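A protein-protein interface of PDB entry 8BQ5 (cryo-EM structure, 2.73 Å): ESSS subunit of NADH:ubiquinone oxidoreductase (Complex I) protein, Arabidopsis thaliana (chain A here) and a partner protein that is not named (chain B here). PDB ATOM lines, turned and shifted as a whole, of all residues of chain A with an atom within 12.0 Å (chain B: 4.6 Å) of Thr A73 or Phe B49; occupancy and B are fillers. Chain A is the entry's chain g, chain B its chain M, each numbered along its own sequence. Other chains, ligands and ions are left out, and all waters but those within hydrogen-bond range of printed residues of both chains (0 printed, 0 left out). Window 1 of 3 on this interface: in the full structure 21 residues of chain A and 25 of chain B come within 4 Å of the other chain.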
ATOM      1  N   TRP A  62      18.449   3.142  26.734  1.00  0.00           N
ATOM      2  CA  TRP A  62      17.496   4.243  26.751  1.00  0.00           C
ATOM      3  C   TRP A  62      18.148   5.597  27.006  1.00  0.00           C
ATOM      4  O   TRP A  62      17.535   6.625  26.703  1.00  0.00           O
ATOM      5  CB  TRP A  62      16.425   3.986  27.812  1.00  0.00           C
ATOM      6  CG  TRP A  62      16.997   3.828  29.177  1.00  0.00           C
ATOM      7  CD1 TRP A  62      17.368   2.665  29.780  1.00  0.00           C
ATOM      8  CD2 TRP A  62      17.274   4.872  30.116  1.00  0.00           C
ATOM      9  NE1 TRP A  62      17.861   2.917  31.034  1.00  0.00           N
ATOM     10  CE2 TRP A  62      17.812   4.267  31.265  1.00  0.00           C
ATOM     11  CE3 TRP A  62      17.116   6.261  30.096  1.00  0.00           C
ATOM     12  CZ2 TRP A  62      18.201   4.999  32.379  1.00  0.00           C
ATOM     13  CZ3 TRP A  62      17.499   6.988  31.205  1.00  0.00           C
ATOM     14  CH2 TRP A  62      18.032   6.355  32.333  1.00  0.00           C
ATOM     15  N   GLU A  63      19.368   5.623  27.546  1.00  0.00           N
ATOM     16  CA  GLU A  63      19.942   6.873  28.039  1.00  0.00           C
ATOM     17  C   GLU A  63      20.195   7.862  26.908  1.00  0.00           C
ATOM     18  O   GLU A  63      19.789   9.027  26.986  1.00  0.00           O
ATOM     19  CB  GLU A  63      21.233   6.589  28.807  1.00  0.00           C
ATOM     20  CG  GLU A  63      21.035   5.691  30.010  1.00  0.00           C
ATOM     21  CD  GLU A  63      22.028   5.968  31.117  1.00  0.00           C
ATOM     22  OE1 GLU A  63      22.282   7.156  31.410  1.00  0.00           O
ATOM     23  OE2 GLU A  63      22.557   4.996  31.692  1.00  0.00           O
ATOM     24  N   LEU A  64      20.866   7.420  25.846  1.00  0.00           N
ATOM     25  CA  LEU A  64      21.192   8.335  24.753  1.00  0.00           C
ATOM     26  C   LEU A  64      19.960   8.913  24.068  1.00  0.00           C
ATOM     27  O   LEU A  64      19.891  10.145  23.916  1.00  0.00           O
ATOM     28  CB  LEU A  64      22.112   7.635  23.745  1.00  0.00           C
ATOM     29  CG  LEU A  64      22.789   8.556  22.729  1.00  0.00           C
ATOM     30  CD1 LEU A  64      23.379   9.779  23.417  1.00  0.00           C
ATOM     31  CD2 LEU A  64      23.850   7.808  21.935  1.00  0.00           C
ATOM     32  N   PRO A  65      18.971   8.120  23.627  1.00  0.00           N
ATOM     33  CA  PRO A  65      17.784   8.739  23.010  1.00  0.00           C
ATOM     34  C   PRO A  65      17.021   9.650  23.955  1.00  0.00           C
ATOM     35  O   PRO A  65      16.469  10.667  23.521  1.00  0.00           O
ATOM     36  CB  PRO A  65      16.937   7.534  22.575  1.00  0.00           C
ATOM     37  CG  PRO A  65      17.842   6.358  22.635  1.00  0.00           C
ATOM     38  CD  PRO A  65      18.854   6.653  23.677  1.00  0.00           C
ATOM     39  N   CYS A  66      16.976   9.310  25.245  1.00  0.00           N
ATOM     40  CA  CYS A  66      16.272  10.153  26.205  1.00  0.00           C
ATOM     41  C   CYS A  66      17.039  11.439  26.480  1.00  0.00           C
ATOM     42  O   CYS A  66      16.434  12.503  26.650  1.00  0.00           O
ATOM     43  CB  CYS A  66      16.032   9.382  27.501  1.00  0.00           C
ATOM     44  SG  CYS A  66      14.595   8.289  27.474  1.00  0.00           S
ATOM     45  N   TYR A  67      18.371  11.363  26.533  1.00  0.00           N
ATOM     46  CA  TYR A  67      19.162  12.562  26.791  1.00  0.00           C
ATOM     47  C   TYR A  67      19.159  13.494  25.586  1.00  0.00           C
ATOM     48  O   TYR A  67      19.118  14.719  25.743  1.00  0.00           O
ATOM     49  CB  TYR A  67      20.592  12.180  27.167  1.00  0.00           C
ATOM     50  CG  TYR A  67      20.711  11.482  28.502  1.00  0.00           C
ATOM     51  CD1 TYR A  67      19.675  11.524  29.423  1.00  0.00           C
ATOM     52  CD2 TYR A  67      21.857  10.777  28.837  1.00  0.00           C
ATOM     53  CE1 TYR A  67      19.777  10.885  30.639  1.00  0.00           C
ATOM     54  CE2 TYR A  67      21.969  10.136  30.051  1.00  0.00           C
ATOM     55  CZ  TYR A  67      20.925  10.194  30.949  1.00  0.00           C
ATOM     56  OH  TYR A  67      21.028   9.559  32.163  1.00  0.00           O
ATOM     57  N   ILE A  68      19.207  12.931  24.378  1.00  0.00           N
ATOM     58  CA  ILE A  68      19.148  13.747  23.170  1.00  0.00           C
ATOM     59  C   ILE A  68      17.796  14.442  23.061  1.00  0.00           C
ATOM     60  O   ILE A  68      17.720  15.632  22.737  1.00  0.00           O
ATOM     61  CB  ILE A  68      19.450  12.884  21.932  1.00  0.00           C
ATOM     62  CG1 ILE A  68      20.919  12.458  21.932  1.00  0.00           C
ATOM     63  CG2 ILE A  68      19.118  13.635  20.657  1.00  0.00           C
ATOM     64  CD1 ILE A  68      21.250  11.424  20.887  1.00  0.00           C
ATOM     65  N   THR A  69      16.710  13.713  23.333  1.00  0.00           N
ATOM     66  CA  THR A  69      15.383  14.317  23.288  1.00  0.00           C
ATOM     67  C   THR A  69      15.242  15.410  24.339  1.00  0.00           C
ATOM     68  O   THR A  69      14.644  16.461  24.078  1.00  0.00           O
ATOM     69  CB  THR A  69      14.312  13.244  23.485  1.00  0.00           C
ATOM     70  OG1 THR A  69      14.287  12.379  22.343  1.00  0.00           O
ATOM     71  CG2 THR A  69      12.942  13.881  23.654  1.00  0.00           C
ATOM     72  N   SER A  70      15.795  15.181  25.533  1.00  0.00           N
ATOM     73  CA  SER A  70      15.732  16.187  26.587  1.00  0.00           C
ATOM     74  C   SER A  70      16.438  17.469  26.169  1.00  0.00           C
ATOM     75  O   SER A  70      15.934  18.568  26.418  1.00  0.00           O
ATOM     76  CB  SER A  70      16.343  15.634  27.873  1.00  0.00           C
ATOM     77  OG  SER A  70      15.544  14.597  28.408  1.00  0.00           O
ATOM     78  N   PHE A  71      17.609  17.349  25.541  1.00  0.00           N
ATOM     79  CA  PHE A  71      18.305  18.530  25.038  1.00  0.00           C
ATOM     80  C   PHE A  71      17.497  19.232  23.955  1.00  0.00           C
ATOM     81  O   PHE A  71      17.388  20.463  23.952  1.00  0.00           O
ATOM     82  CB  PHE A  71      19.680  18.143  24.501  1.00  0.00           C
ATOM     83  CG  PHE A  71      20.379  19.258  23.785  1.00  0.00           C
ATOM     84  CD1 PHE A  71      20.879  20.341  24.484  1.00  0.00           C
ATOM     85  CD2 PHE A  71      20.516  19.233  22.407  1.00  0.00           C
ATOM     86  CE1 PHE A  71      21.516  21.373  23.825  1.00  0.00           C
ATOM     87  CE2 PHE A  71      21.150  20.262  21.743  1.00  0.00           C
ATOM     88  CZ  PHE A  71      21.651  21.335  22.454  1.00  0.00           C
ATOM     89  N   LEU A  72      16.933  18.466  23.019  1.00  0.00           N
ATOM     90  CA  LEU A  72      16.091  19.065  21.989  1.00  0.00           C
ATOM     91  C   LEU A  72      14.865  19.725  22.606  1.00  0.00           C
ATOM     92  O   LEU A  72      14.470  20.819  22.194  1.00  0.00           O
ATOM     93  CB  LEU A  72      15.672  18.008  20.967  1.00  0.00           C
ATOM     94  CG  LEU A  72      16.735  17.503  19.991  1.00  0.00           C
ATOM     95  CD1 LEU A  72      16.147  16.430  19.094  1.00  0.00           C
ATOM     96  CD2 LEU A  72      17.293  18.645  19.162  1.00  0.00           C
ATOM     97  N   THR A  73      14.265  19.078  23.605  1.00  0.00           N
ATOM     98  CA  THR A  73      13.094  19.640  24.269  1.00  0.00           C
ATOM     99  C   THR A  73      13.407  21.003  24.874  1.00  0.00           C
ATOM    100  O   THR A  73      12.575  21.916  24.844  1.00  0.00           O
ATOM    101  CB  THR A  73      12.599  18.675  25.347  1.00  0.00           C
ATOM    102  OG1 THR A  73      12.548  17.347  24.813  1.00  0.00           O
ATOM    103  CG2 THR A  73      11.221  19.075  25.832  1.00  0.00           C
ATOM    104  N   ILE A  74      14.606  21.154  25.439  1.00  0.00           N
ATOM    105  CA  ILE A  74      14.996  22.432  26.029  1.00  0.00           C
ATOM    106  C   ILE A  74      15.238  23.473  24.942  1.00  0.00           C
ATOM    107  O   ILE A  74      14.855  24.640  25.081  1.00  0.00           O
ATOM    108  CB  ILE A  74      16.232  22.252  26.929  1.00  0.00           C
ATOM    109  CG1 ILE A  74      15.979  21.162  27.972  1.00  0.00           C
ATOM    110  CG2 ILE A  74      16.603  23.564  27.598  1.00  0.00           C
ATOM    111  CD1 ILE A  74      15.372  21.660  29.262  1.00  0.00           C
ATOM    112  N   VAL A  75      15.885  23.071  23.845  1.00  0.00           N
ATOM    113  CA  VAL A  75      16.239  24.035  22.804  1.00  0.00           C
ATOM    114  C   VAL A  75      15.010  24.429  21.985  1.00  0.00           C
ATOM    115  O   VAL A  75      14.861  25.589  21.587  1.00  0.00           O
ATOM    116  CB  VAL A  75      17.379  23.488  21.921  1.00  0.00           C
ATOM    117  CG1 VAL A  75      16.873  22.492  20.886  1.00  0.00           C
ATOM    118  CG2 VAL A  75      18.105  24.632  21.236  1.00  0.00           C
ATOM    119  N   ILE A  76      14.112  23.475  21.723  1.00  0.00           N
ATOM    120  CA  ILE A  76      12.929  23.772  20.915  1.00  0.00           C
ATOM    121  C   ILE A  76      11.966  24.661  21.693  1.00  0.00           C
ATOM    122  O   ILE A  76      11.276  25.512  21.122  1.00  0.00           O
ATOM    123  CB  ILE A  76      12.251  22.471  20.445  1.00  0.00           C
ATOM    124  CG1 ILE A  76      13.192  21.676  19.534  1.00  0.00           C
ATOM    125  CG2 ILE A  76      10.932  22.763  19.736  1.00  0.00           C
ATOM    126  CD1 ILE A  76      12.963  21.891  18.052  1.00  0.00           C
ATOM    127  N   LEU A  77      11.913  24.480  23.014  1.00  0.00           N
ATOM    128  CA  LEU A  77      10.989  25.259  23.831  1.00  0.00           C
ATOM    129  C   LEU A  77      11.660  26.508  24.388  1.00  0.00           C
ATOM    130  O   LEU A  77      11.051  27.583  24.433  1.00  0.00           O
ATOM    131  CB  LEU A  77      10.435  24.396  24.964  1.00  0.00           C
ATOM    132  CG  LEU A  77       9.405  23.339  24.567  1.00  0.00           C
ATOM    133  CD1 LEU A  77       8.876  22.623  25.798  1.00  0.00           C
ATOM    134  CD2 LEU A  77       8.268  23.979  23.788  1.00  0.00           C
ATOM    135  N   GLY A  78      12.913  26.387  24.830  1.00  0.00           N
ATOM    136  CA  GLY A  78      13.600  27.536  25.394  1.00  0.00           C
ATOM    137  C   GLY A  78      13.863  28.631  24.381  1.00  0.00           C
ATOM    138  O   GLY A  78      13.812  29.817  24.715  1.00  0.00           O
ATOM    139  N   VAL A  79      14.149  28.255  23.140  1.00  0.00           N
ATOM    140  CA  VAL A  79      14.387  29.221  22.072  1.00  0.00           C
ATOM    141  C   VAL A  79      13.125  29.463  21.256  1.00  0.00           C
ATOM    142  O   VAL A  79      12.845  30.591  20.843  1.00  0.00           O
ATOM    143  CB  VAL A  79      15.554  28.736  21.186  1.00  0.00           C
ATOM    144  CG1 VAL A  79      15.662  29.571  19.916  1.00  0.00           C
ATOM    145  CG2 VAL A  79      16.857  28.772  21.966  1.00  0.00           C
ATOM    146  N   GLY A  80      12.346  28.409  21.013  1.00  0.00           N
ATOM    147  CA  GLY A  80      11.157  28.555  20.189  1.00  0.00           C
ATOM    148  C   GLY A  80      10.084  29.416  20.829  1.00  0.00           C
ATOM    149  O   GLY A  80       9.462  30.244  20.158  1.00  0.00           O
ATOM    150  N   LEU A  81       9.841  29.228  22.127  1.00  0.00           N
ATOM    151  CA  LEU A  81       8.790  29.991  22.791  1.00  0.00           C
ATOM    152  C   LEU A  81       9.160  31.464  22.897  1.00  0.00           C
ATOM    153  O   LEU A  81       8.289  32.337  22.800  1.00  0.00           O
ATOM    154  CB  LEU A  81       8.506  29.406  24.176  1.00  0.00           C
ATOM    155  CG  LEU A  81       7.782  28.057  24.226  1.00  0.00           C
ATOM    156  CD1 LEU A  81       7.496  27.660  25.665  1.00  0.00           C
ATOM    157  CD2 LEU A  81       6.503  28.082  23.407  1.00  0.00           C
ATOM    158  N   ASN A  82      10.444  31.762  23.095  1.00  0.00           N
ATOM    159  CA  ASN A  82      10.919  33.136  23.196  1.00  0.00           C
ATOM    160  C   ASN A  82      11.063  33.820  21.845  1.00  0.00           C
ATOM    161  O   ASN A  82      11.169  35.050  21.802  1.00  0.00           O
ATOM    162  CB  ASN A  82      12.264  33.174  23.921  1.00  0.00           C
ATOM    163  CG  ASN A  82      12.143  32.821  25.383  1.00  0.00           C
ATOM    164  OD1 ASN A  82      11.665  33.617  26.188  1.00  0.00           O
ATOM    165  ND2 ASN A  82      12.569  31.614  25.737  1.00  0.00           N
ATOM    166  N   ALA A  83      11.079  33.064  20.748  1.00  0.00           N
ATOM    167  CA  ALA A  83      11.238  33.642  19.423  1.00  0.00           C
ATOM    168  C   ALA A  83       9.933  33.758  18.655  1.00  0.00           C
ATOM    169  O   ALA A  83       9.871  34.517  17.683  1.00  0.00           O
ATOM    170  CB  ALA A  83      12.222  32.811  18.596  1.00  0.00           C
ATOM    171  N   SER B  45       8.232   7.047  19.712  1.00  0.00           N
ATOM    172  CA  SER B  45       7.480   7.881  20.647  1.00  0.00           C
ATOM    173  C   SER B  45       8.170   9.223  20.876  1.00  0.00           C
ATOM    174  O   SER B  45       7.509  10.269  20.946  1.00  0.00           O
ATOM    175  CB  SER B  45       7.281   7.139  21.969  1.00  0.00           C
ATOM    176  OG  SER B  45       8.520   6.740  22.523  1.00  0.00           O
ATOM    177  N   LEU B  46       9.502   9.215  20.989  1.00  0.00           N
ATOM    178  CA  LEU B  46      10.236  10.459  21.199  1.00  0.00           C
ATOM    179  C   LEU B  46      10.108  11.395  20.001  1.00  0.00           C
ATOM    180  O   LEU B  46       9.942  12.613  20.167  1.00  0.00           O
ATOM    181  CB  LEU B  46      11.705  10.151  21.486  1.00  0.00           C
ATOM    182  CG  LEU B  46      11.991   9.526  22.851  1.00  0.00           C
ATOM    183  CD1 LEU B  46      13.450   9.112  22.964  1.00  0.00           C
ATOM    184  CD2 LEU B  46      11.601  10.471  23.972  1.00  0.00           C
ATOM    185  N   ILE B  47      10.191  10.846  18.786  1.00  0.00           N
ATOM    186  CA  ILE B  47      10.022  11.662  17.587  1.00  0.00           C
ATOM    187  C   ILE B  47       8.630  12.275  17.559  1.00  0.00           C
ATOM    188  O   ILE B  47       8.455  13.444  17.188  1.00  0.00           O
ATOM    189  CB  ILE B  47      10.304  10.821  16.326  1.00  0.00           C
ATOM    190  CG1 ILE B  47      11.800  10.534  16.195  1.00  0.00           C
ATOM    191  CG2 ILE B  47       9.794  11.521  15.076  1.00  0.00           C
ATOM    192  CD1 ILE B  47      12.108   9.291  15.395  1.00  0.00           C
ATOM    193  N   THR B  48       7.616  11.500  17.955  1.00  0.00           N
ATOM    194  CA  THR B  48       6.258  12.036  18.014  1.00  0.00           C
ATOM    195  C   THR B  48       6.157  13.191  19.007  1.00  0.00           C
ATOM    196  O   THR B  48       5.512  14.212  18.725  1.00  0.00           O
ATOM    197  CB  THR B  48       5.277  10.922  18.378  1.00  0.00           C
ATOM    198  OG1 THR B  48       5.719   9.690  17.796  1.00  0.00           O
ATOM    199  CG2 THR B  48       3.886  11.246  17.865  1.00  0.00           C
ATOM    200  N   PHE B  49       6.787  13.048  20.176  1.00  0.00           N
ATOM    201  CA  PHE B  49       6.766  14.127  21.164  1.00  0.00           C
ATOM    202  C   PHE B  49       7.409  15.396  20.611  1.00  0.00           C
ATOM    203  O   PHE B  49       6.879  16.505  20.781  1.00  0.00           O
ATOM    204  CB  PHE B  49       7.480  13.677  22.439  1.00  0.00           C
ATOM    205  CG  PHE B  49       7.628  14.757  23.473  1.00  0.00           C
ATOM    206  CD1 PHE B  49       6.513  15.359  24.028  1.00  0.00           C
ATOM    207  CD2 PHE B  49       8.881  15.166  23.893  1.00  0.00           C
ATOM    208  CE1 PHE B  49       6.646  16.348  24.984  1.00  0.00           C
ATOM    209  CE2 PHE B  49       9.022  16.153  24.844  1.00  0.00           C
ATOM    210  CZ  PHE B  49       7.904  16.747  25.391  1.00  0.00           C
ATOM    211  N   LEU B  50       8.552  15.250  19.935  1.00  0.00           N
ATOM    212  CA  LEU B  50       9.218  16.414  19.357  1.00  0.00           C
ATOM    213  C   LEU B  50       8.354  17.071  18.283  1.00  0.00           C
ATOM    214  O   LEU B  50       8.277  18.305  18.199  1.00  0.00           O
ATOM    215  CB  LEU B  50      10.573  16.002  18.786  1.00  0.00           C
ATOM    216  CG  LEU B  50      11.583  15.545  19.840  1.00  0.00           C
ATOM    217  CD1 LEU B  50      12.811  14.941  19.183  1.00  0.00           C
ATOM    218  CD2 LEU B  50      11.964  16.695  20.757  1.00  0.00           C
ATOM    219  N   TYR B  51       7.696  16.256  17.455  1.00  0.00           N
ATOM    220  CA  TYR B  51       6.786  16.784  16.444  1.00  0.00           C
ATOM    221  C   TYR B  51       5.670  17.599  17.086  1.00  0.00           C
ATOM    222  O   TYR B  51       5.312  18.676  16.592  1.00  0.00           O
ATOM    223  CB  TYR B  51       6.215  15.624  15.625  1.00  0.00           C
ATOM    224  CG  TYR B  51       5.615  15.995  14.286  1.00  0.00           C
ATOM    225  CD1 TYR B  51       4.524  16.850  14.198  1.00  0.00           C
ATOM    226  CD2 TYR B  51       6.132  15.473  13.109  1.00  0.00           C
ATOM    227  CE1 TYR B  51       3.977  17.182  12.982  1.00  0.00           C
ATOM    228  CE2 TYR B  51       5.589  15.799  11.885  1.00  0.00           C
ATOM    229  CZ  TYR B  51       4.510  16.654  11.828  1.00  0.00           C
ATOM    230  OH  TYR B  51       3.964  16.983  10.611  1.00  0.00           O
ATOM    231  N   SER B  52       5.105  17.096  18.186  1.00  0.00           N
ATOM    232  CA  SER B  52       4.052  17.839  18.875  1.00  0.00           C
ATOM    233  C   SER B  52       4.575  19.163  19.420  1.00  0.00           C
ATOM    234  O   SER B  52       3.862  20.177  19.407  1.00  0.00           O
ATOM    235  CB  SER B  52       3.459  16.994  20.000  1.00  0.00           C
ATOM    236  OG  SER B  52       4.172  17.182  21.208  1.00  0.00           O
ATOM    237  N   LEU B  53       5.813  19.176  19.914  1.00  0.00           N
ATOM    238  CA  LEU B  53       6.386  20.437  20.379  1.00  0.00           C
ATOM    239  C   LEU B  53       6.516  21.437  19.233  1.00  0.00           C
ATOM    240  O   LEU B  53       6.233  22.633  19.402  1.00  0.00           O
ATOM    241  CB  LEU B  53       7.740  20.194  21.039  1.00  0.00           C
ATOM    242  CG  LEU B  53       7.694  19.480  22.392  1.00  0.00           C
ATOM    243  CD1 LEU B  53       9.020  19.640  23.107  1.00  0.00           C
ATOM    244  CD2 LEU B  53       6.538  19.967  23.256  1.00  0.00           C
ATOM    245  N   ILE B  95      -0.127  17.478  23.098  1.00  0.00           N
ATOM    246  CA  ILE B  95       1.243  17.485  23.610  1.00  0.00           C
ATOM    247  C   ILE B  95       1.370  16.560  24.820  1.00  0.00           C
ATOM    248  O   ILE B  95       2.366  15.842  24.969  1.00  0.00           O
ATOM    249  CB  ILE B  95       1.692  18.922  23.931  1.00  0.00           C
ATOM    250  CG1 ILE B  95       1.825  19.732  22.644  1.00  0.00           C
ATOM    251  CG2 ILE B  95       3.028  18.922  24.647  1.00  0.00           C
ATOM    252  CD1 ILE B  95       2.005  21.205  22.880  1.00  0.00           C
ATOM    253  N   THR B  98       1.450  12.879  23.674  1.00  0.00           N
ATOM    254  CA  THR B  98       2.752  12.550  23.103  1.00  0.00           C
ATOM    255  C   THR B  98       3.840  12.525  24.164  1.00  0.00           C
ATOM    256  O   THR B  98       4.880  11.891  23.965  1.00  0.00           O
ATOM    257  CB  THR B  98       3.123  13.552  22.012  1.00  0.00           C
ATOM    258  OG1 THR B  98       3.086  14.878  22.549  1.00  0.00           O
ATOM    259  CG2 THR B  98       2.146  13.462  20.857  1.00  0.00           C
ATOM    260  N   PHE B  99       3.648  13.245  25.268  1.00  0.00           N
ATOM    261  CA  PHE B  99       4.618  13.188  26.354  1.00  0.00           C
ATOM    262  C   PHE B  99       4.450  11.927  27.195  1.00  0.00           C
ATOM    263  O   PHE B  99       5.438  11.355  27.667  1.00  0.00           O
ATOM    264  CB  PHE B  99       4.494  14.431  27.235  1.00  0.00           C
ATOM    265  CG  PHE B  99       5.038  14.247  28.620  1.00  0.00           C
ATOM    266  CD1 PHE B  99       6.403  14.197  28.838  1.00  0.00           C
ATOM    267  CD2 PHE B  99       4.186  14.122  29.703  1.00  0.00           C
ATOM    268  CE1 PHE B  99       6.907  14.027  30.109  1.00  0.00           C
ATOM    269  CE2 PHE B  99       4.687  13.950  30.977  1.00  0.00           C
ATOM    270  CZ  PHE B  99       6.047  13.906  31.182  1.00  0.00           C
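O of Pro A65 sits at hydrogen-bond distance from OG1 of Thr A69.
The side-chain hydroxyl (OG) of Ser B52 lies within hydrogen-bond range of the backbone carbonyl oxygen (O) of Phe B49 (2.8 Å).
Among the printed residues, pairs that only touch across the chains: Pro A65 with Leu B46 (3.4 Å), Thr A69 with Leu B46 (3.4 Å), Leu A72 with Leu B50 (3.7 Å), Thr A73 with Phe B49 (3.7 Å), Thr A73 with Leu B53 (3.5 Å) and Leu A77 with Leu B53 (3.995 Å).
Of chain B, only Phe B49 (3.7 Å) and Leu B53 (3.5 Å) come within 4 Å of Thr A73.
Of chain A, only Thr A73 comes within 4 Å of Phe B49.
Of chain A, only Pro A65 (3.4 Å) and Thr A69 (3.4 Å) come within 4 Å of Leu B46.
No residue of chain A comes within 4 Å of Thr B48.
Leu B50 touches just one residue of chain A: Leu A72 (3.7 Å).
No residue of chain A comes within 4 Å of Ile B95.
Thr B98 touches none of the printed residues of chain A.
No residue of chain A comes within 4 Å of Phe B99.
Printed residues of chain B within 4 Å of Leu A77: Leu B53 (3.995 Å).
Of the printed residues of chain B, Thr A69 touches Leu B46 (3.4 Å).
Of the printed residues of chain B, Pro A65 touches Leu B46.
Of the printed residues of chain A, Leu B53 touches Thr A73 (3.5 Å) and Leu A77 (3.995 Å).
Printed residues of chain B within 4 Å of Leu A72: Leu B50.
The nearest residue of chain B that does not touch Thr A73 is Leu B50 (4.1 Å).
The nearest residue of chain A that does not touch Phe B49 is Thr A69 (4.3 Å).
Hydrophobic or aromatic side chains of chain A that line the printed part of chain B: Pro A65, Leu A72 and Leu A77.
Printed residues of chain B that touch a printed residue of chain A: Leu B46, Phe B49, Leu B50 and Leu B53.
Hydrophobic or aromatic side chains of chain B within 4 Å of the printed part of chain A: Leu B46, Phe B49, Leu B50 and Leu B53.
Among the printed residues, no Asp or Glu carboxylate lies within 4 Å of a Lys or Arg side-chain nitrogen of the other chain.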
